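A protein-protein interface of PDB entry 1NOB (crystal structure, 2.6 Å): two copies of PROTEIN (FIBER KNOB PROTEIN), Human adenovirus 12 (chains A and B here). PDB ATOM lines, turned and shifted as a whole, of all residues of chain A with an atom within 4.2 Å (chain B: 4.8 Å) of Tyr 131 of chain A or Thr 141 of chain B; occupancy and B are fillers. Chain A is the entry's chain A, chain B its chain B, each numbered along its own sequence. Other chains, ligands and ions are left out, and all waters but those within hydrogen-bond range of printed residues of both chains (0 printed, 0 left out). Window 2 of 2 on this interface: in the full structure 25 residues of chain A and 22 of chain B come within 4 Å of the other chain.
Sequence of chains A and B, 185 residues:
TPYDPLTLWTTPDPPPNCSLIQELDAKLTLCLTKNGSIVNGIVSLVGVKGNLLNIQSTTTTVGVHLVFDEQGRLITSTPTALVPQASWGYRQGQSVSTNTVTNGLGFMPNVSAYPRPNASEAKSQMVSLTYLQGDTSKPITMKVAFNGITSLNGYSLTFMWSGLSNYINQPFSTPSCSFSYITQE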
ATOM      1  N   THR A 130     -15.861  14.190  20.611  1.00  0.00           N
ATOM      2  CA  THR A 130     -16.299  12.807  20.510  1.00  0.00           C
ATOM      3  C   THR A 130     -17.825  12.767  20.297  1.00  0.00           C
ATOM      4  O   THR A 130     -18.462  13.817  20.150  1.00  0.00           O
ATOM      5  CB  THR A 130     -15.871  12.009  21.744  1.00  0.00           C
ATOM      6  OG1 THR A 130     -16.122  10.621  21.510  1.00  0.00           O
ATOM      7  CG2 THR A 130     -16.625  12.466  22.988  1.00  0.00           C
ATOM      8  N   TYR A 131     -18.424  11.580  20.278  1.00  0.00           N
ATOM      9  CA  TYR A 131     -19.851  11.515  20.001  1.00  0.00           C
ATOM     10  C   TYR A 131     -20.765  10.725  20.930  1.00  0.00           C
ATOM     11  O   TYR A 131     -20.544   9.537  21.181  1.00  0.00           O
ATOM     12  CB  TYR A 131     -20.052  11.028  18.570  1.00  0.00           C
ATOM     13  CG  TYR A 131     -19.313  11.848  17.547  1.00  0.00           C
ATOM     14  CD1 TYR A 131     -17.952  11.661  17.315  1.00  0.00           C
ATOM     15  CD2 TYR A 131     -19.977  12.810  16.803  1.00  0.00           C
ATOM     16  CE1 TYR A 131     -17.277  12.411  16.356  1.00  0.00           C
ATOM     17  CE2 TYR A 131     -19.315  13.563  15.847  1.00  0.00           C
ATOM     18  CZ  TYR A 131     -17.973  13.359  15.630  1.00  0.00           C
ATOM     19  OH  TYR A 131     -17.344  14.122  14.683  1.00  0.00           O
ATOM     20  N   LEU A 132     -21.806  11.399  21.418  1.00  0.00           N
ATOM     21  CA  LEU A 132     -22.794  10.804  22.325  1.00  0.00           C
ATOM     22  C   LEU A 132     -23.392   9.513  21.763  1.00  0.00           C
ATOM     23  O   LEU A 132     -24.023   9.512  20.703  1.00  0.00           O
ATOM     24  CB  LEU A 132     -23.912  11.808  22.584  1.00  0.00           C
ATOM     25  CG  LEU A 132     -25.119  11.344  23.380  1.00  0.00           C
ATOM     26  CD1 LEU A 132     -24.666  10.788  24.726  1.00  0.00           C
ATOM     27  CD2 LEU A 132     -26.083  12.511  23.547  1.00  0.00           C
ATOM     28  N   GLN A 133     -23.193   8.416  22.479  1.00  0.00           N
ATOM     29  CA  GLN A 133     -23.696   7.125  22.035  1.00  0.00           C
ATOM     30  C   GLN A 133     -22.878   6.633  20.844  1.00  0.00           C
ATOM     31  O   GLN A 133     -23.097   5.533  20.355  1.00  0.00           O
ATOM     32  CB  GLN A 133     -25.174   7.254  21.663  1.00  0.00           C
ATOM     33  CG  GLN A 133     -26.011   7.766  22.814  1.00  0.00           C
ATOM     34  CD  GLN A 133     -27.388   8.229  22.392  1.00  0.00           C
ATOM     35  OE1 GLN A 133     -28.187   8.654  23.233  1.00  0.00           O
ATOM     36  NE2 GLN A 133     -27.675   8.163  21.090  1.00  0.00           N
ATOM     37  N   GLY A 134     -21.931   7.453  20.393  1.00  0.00           N
ATOM     38  CA  GLY A 134     -21.080   7.084  19.269  1.00  0.00           C
ATOM     39  C   GLY A 134     -21.755   7.344  17.940  1.00  0.00           C
ATOM     40  O   GLY A 134     -21.460   6.700  16.940  1.00  0.00           O
ATOM     41  N   ASP A 135     -22.664   8.309  17.957  1.00  0.00           N
ATOM     42  CA  ASP A 135     -23.465   8.712  16.812  1.00  0.00           C
ATOM     43  C   ASP A 135     -22.796   9.928  16.186  1.00  0.00           C
ATOM     44  O   ASP A 135     -22.779  11.000  16.793  1.00  0.00           O
ATOM     45  CB  ASP A 135     -24.878   9.037  17.325  1.00  0.00           C
ATOM     46  CG  ASP A 135     -25.822   9.508  16.243  1.00  0.00           C
ATOM     47  OD1 ASP A 135     -25.358   9.954  15.169  1.00  0.00           O
ATOM     48  OD2 ASP A 135     -27.049   9.450  16.493  1.00  0.00           O
ATOM     49  N   THR A 136     -22.251   9.758  14.977  1.00  0.00           N
ATOM     50  CA  THR A 136     -21.535  10.845  14.298  1.00  0.00           C
ATOM     51  C   THR A 136     -22.325  12.115  14.039  1.00  0.00           C
ATOM     52  O   THR A 136     -21.847  13.006  13.353  1.00  0.00           O
ATOM     53  CB  THR A 136     -20.911  10.396  12.942  1.00  0.00           C
ATOM     54  OG1 THR A 136     -21.929   9.838  12.091  1.00  0.00           O
ATOM     55  CG2 THR A 136     -19.797   9.386  13.178  1.00  0.00           C
ATOM     56  N   LYS A 138     -24.132  13.311  16.803  1.00  0.00           N
ATOM     57  CA  LYS A 138     -24.295  13.815  18.157  1.00  0.00           C
ATOM     58  C   LYS A 138     -22.960  14.080  18.826  1.00  0.00           C
ATOM     59  O   LYS A 138     -22.611  13.418  19.798  1.00  0.00           O
ATOM     60  CB  LYS A 138     -25.098  12.820  18.991  1.00  0.00           C
ATOM     61  CG  LYS A 138     -26.487  12.540  18.445  1.00  0.00           C
ATOM     62  CD  LYS A 138     -27.191  11.515  19.298  1.00  0.00           C
ATOM     63  CE  LYS A 138     -28.530  11.102  18.722  1.00  0.00           C
ATOM     64  NZ  LYS A 138     -29.115  10.035  19.576  1.00  0.00           N
ATOM     65  N   PRO A 139     -22.177  15.026  18.286  1.00  0.00           N
ATOM     66  CA  PRO A 139     -20.869  15.398  18.824  1.00  0.00           C
ATOM     67  C   PRO A 139     -20.919  16.014  20.204  1.00  0.00           C
ATOM     68  O   PRO A 139     -21.887  16.682  20.566  1.00  0.00           O
ATOM     69  CB  PRO A 139     -20.354  16.392  17.791  1.00  0.00           C
ATOM     70  CG  PRO A 139     -21.628  17.017  17.304  1.00  0.00           C
ATOM     71  CD  PRO A 139     -22.422  15.782  17.045  1.00  0.00           C
ATOM     72  N   ILE A 140     -19.856  15.789  20.965  1.00  0.00           N
ATOM     73  CA  ILE A 140     -19.713  16.329  22.315  1.00  0.00           C
ATOM     74  C   ILE A 140     -18.228  16.409  22.603  1.00  0.00           C
ATOM     75  O   ILE A 140     -17.405  16.096  21.732  1.00  0.00           O
ATOM     76  CB  ILE A 140     -20.351  15.409  23.377  1.00  0.00           C
ATOM     77  CG1 ILE A 140     -19.677  14.032  23.330  1.00  0.00           C
ATOM     78  CG2 ILE A 140     -21.870  15.321  23.159  1.00  0.00           C
ATOM     79  CD1 ILE A 140     -20.307  13.001  24.238  1.00  0.00           C
ATOM     80  N   PRO A 175     -18.750   6.615  23.779  1.00  0.00           N
ATOM     81  CA  PRO A 175     -17.931   5.570  23.178  1.00  0.00           C
ATOM     82  C   PRO A 175     -16.686   5.397  24.059  1.00  0.00           C
ATOM     83  O   PRO A 175     -16.513   6.134  25.029  1.00  0.00           O
ATOM     84  CB  PRO A 175     -17.609   6.164  21.806  1.00  0.00           C
ATOM     85  CG  PRO A 175     -17.500   7.637  22.129  1.00  0.00           C
ATOM     86  CD  PRO A 175     -18.746   7.822  22.928  1.00  0.00           C
ATOM     87  N   VAL B 127     -14.903   7.014  18.440  1.00  0.00           N
ATOM     88  CA  VAL B 127     -15.219   7.915  17.337  1.00  0.00           C
ATOM     89  C   VAL B 127     -14.497   9.257  17.393  1.00  0.00           C
ATOM     90  O   VAL B 127     -14.414   9.892  18.444  1.00  0.00           O
ATOM     91  CB  VAL B 127     -16.754   8.148  17.263  1.00  0.00           C
ATOM     92  CG1 VAL B 127     -17.117   8.846  15.981  1.00  0.00           C
ATOM     93  CG2 VAL B 127     -17.481   6.825  17.363  1.00  0.00           C
ATOM     94  N   SER B 128     -13.976   9.690  16.250  1.00  0.00           N
ATOM     95  CA  SER B 128     -13.269  10.954  16.207  1.00  0.00           C
ATOM     96  C   SER B 128     -13.537  11.741  14.936  1.00  0.00           C
ATOM     97  O   SER B 128     -14.036  11.207  13.955  1.00  0.00           O
ATOM     98  CB  SER B 128     -11.751  10.725  16.351  1.00  0.00           C
ATOM     99  OG  SER B 128     -11.216  10.011  15.242  1.00  0.00           O
ATOM    100  N   LEU B 129     -13.202  13.025  14.981  1.00  0.00           N
ATOM    101  CA  LEU B 129     -13.352  13.912  13.841  1.00  0.00           C
ATOM    102  C   LEU B 129     -11.973  14.103  13.239  1.00  0.00           C
ATOM    103  O   LEU B 129     -11.009  14.382  13.957  1.00  0.00           O
ATOM    104  CB  LEU B 129     -13.885  15.278  14.272  1.00  0.00           C
ATOM    105  CG  LEU B 129     -13.878  16.346  13.175  1.00  0.00           C
ATOM    106  CD1 LEU B 129     -14.768  15.902  12.040  1.00  0.00           C
ATOM    107  CD2 LEU B 129     -14.359  17.678  13.726  1.00  0.00           C
ATOM    108  N   PRO B 139     -13.778  18.263   6.868  1.00  0.00           N
ATOM    109  CA  PRO B 139     -13.959  17.366   8.006  1.00  0.00           C
ATOM    110  C   PRO B 139     -14.728  16.087   7.664  1.00  0.00           C
ATOM    111  O   PRO B 139     -15.606  16.087   6.801  1.00  0.00           O
ATOM    112  CB  PRO B 139     -14.715  18.247   8.989  1.00  0.00           C
ATOM    113  CG  PRO B 139     -15.598  19.027   8.054  1.00  0.00           C
ATOM    114  CD  PRO B 139     -14.559  19.495   7.076  1.00  0.00           C
ATOM    115  N   ILE B 140     -14.377  14.995   8.337  1.00  0.00           N
ATOM    116  CA  ILE B 140     -15.056  13.710   8.150  1.00  0.00           C
ATOM    117  C   ILE B 140     -14.985  12.951   9.458  1.00  0.00           C
ATOM    118  O   ILE B 140     -14.273  13.360  10.361  1.00  0.00           O
ATOM    119  CB  ILE B 140     -14.425  12.874   7.011  1.00  0.00           C
ATOM    120  CG1 ILE B 140     -12.923  12.712   7.229  1.00  0.00           C
ATOM    121  CG2 ILE B 140     -14.725  13.538   5.669  1.00  0.00           C
ATOM    122  CD1 ILE B 140     -12.274  11.861   6.193  1.00  0.00           C
ATOM    123  N   THR B 141     -15.713  11.858   9.582  1.00  0.00           N
ATOM    124  CA  THR B 141     -15.694  11.122  10.847  1.00  0.00           C
ATOM    125  C   THR B 141     -15.143   9.706  10.752  1.00  0.00           C
ATOM    126  O   THR B 141     -15.546   8.951   9.869  1.00  0.00           O
ATOM    127  CB  THR B 141     -17.113  11.039  11.455  1.00  0.00           C
ATOM    128  OG1 THR B 141     -17.994  10.393  10.531  1.00  0.00           O
ATOM    129  CG2 THR B 141     -17.642  12.421  11.752  1.00  0.00           C
ATOM    130  N   MET B 142     -14.230   9.338  11.648  1.00  0.00           N
ATOM    131  CA  MET B 142     -13.684   7.985  11.627  1.00  0.00           C
ATOM    132  C   MET B 142     -14.225   7.177  12.789  1.00  0.00           C
ATOM    133  O   MET B 142     -13.919   7.470  13.944  1.00  0.00           O
ATOM    134  CB  MET B 142     -12.151   7.965  11.720  1.00  0.00           C
ATOM    135  CG  MET B 142     -11.578   6.534  11.640  1.00  0.00           C
ATOM    136  SD  MET B 142      -9.769   6.276  11.848  1.00  0.00           S
ATOM    137  CE  MET B 142      -9.490   6.779  13.543  1.00  0.00           C
ATOM    138  N   LYS B 143     -15.036   6.167  12.488  1.00  0.00           N
ATOM    139  CA  LYS B 143     -15.569   5.305  13.525  1.00  0.00           C
ATOM    140  C   LYS B 143     -14.770   4.026  13.465  1.00  0.00           C
ATOM    141  O   LYS B 143     -14.499   3.501  12.387  1.00  0.00           O
ATOM    142  CB  LYS B 143     -17.040   4.971  13.296  1.00  0.00           C
ATOM    143  CG  LYS B 143     -17.600   4.044  14.377  1.00  0.00           C
ATOM    144  CD  LYS B 143     -19.021   3.568  14.074  1.00  0.00           C
ATOM    145  CE  LYS B 143     -20.004   4.697  14.102  1.00  0.00           C
ATOM    146  NZ  LYS B 143     -20.090   5.242  15.463  1.00  0.00           N
ATOM    147  N   MET B 160     -14.588   3.156   9.757  1.00  0.00           N
ATOM    148  CA  MET B 160     -15.567   3.875   8.977  1.00  0.00           C
ATOM    149  C   MET B 160     -15.269   5.374   8.986  1.00  0.00           C
ATOM    150  O   MET B 160     -15.157   5.993  10.043  1.00  0.00           O
ATOM    151  CB  MET B 160     -16.975   3.621   9.527  1.00  0.00           C
ATOM    152  CG  MET B 160     -17.482   2.194   9.355  1.00  0.00           C
ATOM    153  SD  MET B 160     -17.534   1.718   7.602  1.00  0.00           S
ATOM    154  CE  MET B 160     -18.236   0.021   7.699  1.00  0.00           C
ATOM    155  N   TRP B 161     -15.118   5.937   7.793  1.00  0.00           N
ATOM    156  CA  TRP B 161     -14.883   7.366   7.595  1.00  0.00           C
ATOM    157  C   TRP B 161     -16.131   7.861   6.880  1.00  0.00           C
ATOM    158  O   TRP B 161     -16.334   7.570   5.706  1.00  0.00           O
ATOM    159  CB  TRP B 161     -13.650   7.586   6.722  1.00  0.00           C
ATOM    160  CG  TRP B 161     -12.348   7.295   7.421  1.00  0.00           C
ATOM    161  CD1 TRP B 161     -11.732   8.076   8.353  1.00  0.00           C
ATOM    162  CD2 TRP B 161     -11.530   6.119   7.281  1.00  0.00           C
ATOM    163  NE1 TRP B 161     -10.584   7.463   8.806  1.00  0.00           N
ATOM    164  CE2 TRP B 161     -10.438   6.261   8.165  1.00  0.00           C
ATOM    165  CE3 TRP B 161     -11.618   4.961   6.496  1.00  0.00           C
ATOM    166  CZ2 TRP B 161      -9.441   5.294   8.286  1.00  0.00           C
ATOM    167  CZ3 TRP B 161     -10.625   3.995   6.618  1.00  0.00           C
ATOM    168  CH2 TRP B 161      -9.551   4.171   7.509  1.00  0.00           C
ATOM    169  N   SER B 162     -16.977   8.584   7.606  1.00  0.00           N
ATOM    170  CA  SER B 162     -18.226   9.103   7.056  1.00  0.00           C
ATOM    171  C   SER B 162     -18.133  10.574   6.702  1.00  0.00           C
ATOM    172  O   SER B 162     -17.080  11.184   6.843  1.00  0.00           O
ATOM    173  CB  SER B 162     -19.366   8.906   8.058  1.00  0.00           C
ATOM    174  OG  SER B 162     -19.554   7.536   8.356  1.00  0.00           O
ATOM    175  N   GLY B 163     -19.254  11.137   6.258  1.00  0.00           N
ATOM    176  CA  GLY B 163     -19.292  12.536   5.886  1.00  0.00           C
ATOM    177  C   GLY B 163     -18.404  12.817   4.689  1.00  0.00           C
ATOM    178  O   GLY B 163     -17.534  13.682   4.741  1.00  0.00           O
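Tyr 131 of chain A touches three residues of chain B.
Thr 141 of chain B touches just these residues of chain A: Tyr 131 (3.4 Å) and Thr 136 (3.4 Å).
Printed residues of chain B within 4 Å of Thr 130 of chain A: Val 127 (3.6 Å).
Of the printed residues of chain B, Thr 136 of chain A touches Val 127 (3.9 Å) and Thr 141 (3.4 Å).
The nearest residue of chain B that does not touch Tyr 131 of chain A is Ser 128 of chain B (4.1 Å).
The nearest printed residue of chain A that does not touch Thr 141 of chain B is Asp 135 of chain A (7.2 Å).
The backbone NH (N) of Ile 140 of chain A is in hydrogen-bond range of the backbone carbonyl oxygen (O) of Thr 130 of chain A (2.5 Å).
N of Ser 162 of chain B is in hydrogen-bond range of O of Thr 141 of chain B (2.7 Å).
The backbone NH (N) of Lys 143 of chain B lies within hydrogen-bond range of the backbone carbonyl oxygen (O) of Met 160 of chain B (2.5 Å).
Positions printed for both chains: 139 and 140.
Of the 11 printed residues of chain A, 4 touch a printed residue of chain B.
Hydrophobic or aromatic side chains of chain A within 4 Å of the printed part of chain B: Tyr 131.
Among the printed residues, no Asp or Glu carboxylate lies within 4 Å of a Lys or Arg side-chain nitrogen of the other chain.
The backbone carbonyl oxygen of Gly 134 of chain A sits at hydrogen-bond distance from the side-chain amino group of Lys 143 of chain B, 2.5 Å away.
Thr 130 of chain A touches Val 127 of chain B.
Val 127 of chain B touches Tyr 131 of chain A (CG1 to CD1, 3.2 Å).
Tyr 131 of chain A touches Leu 129 of chain B (OH to CB, 3.7 Å).
Tyr 131 of chain A touches Thr 141 of chain B (OH to CG2, 3.4 Å).
CG1 of Val 127 of chain B touches CG2 of Thr 136 of chain A, at 3.9 Å.
Thr 136 of chain A touches Thr 141 of chain B.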
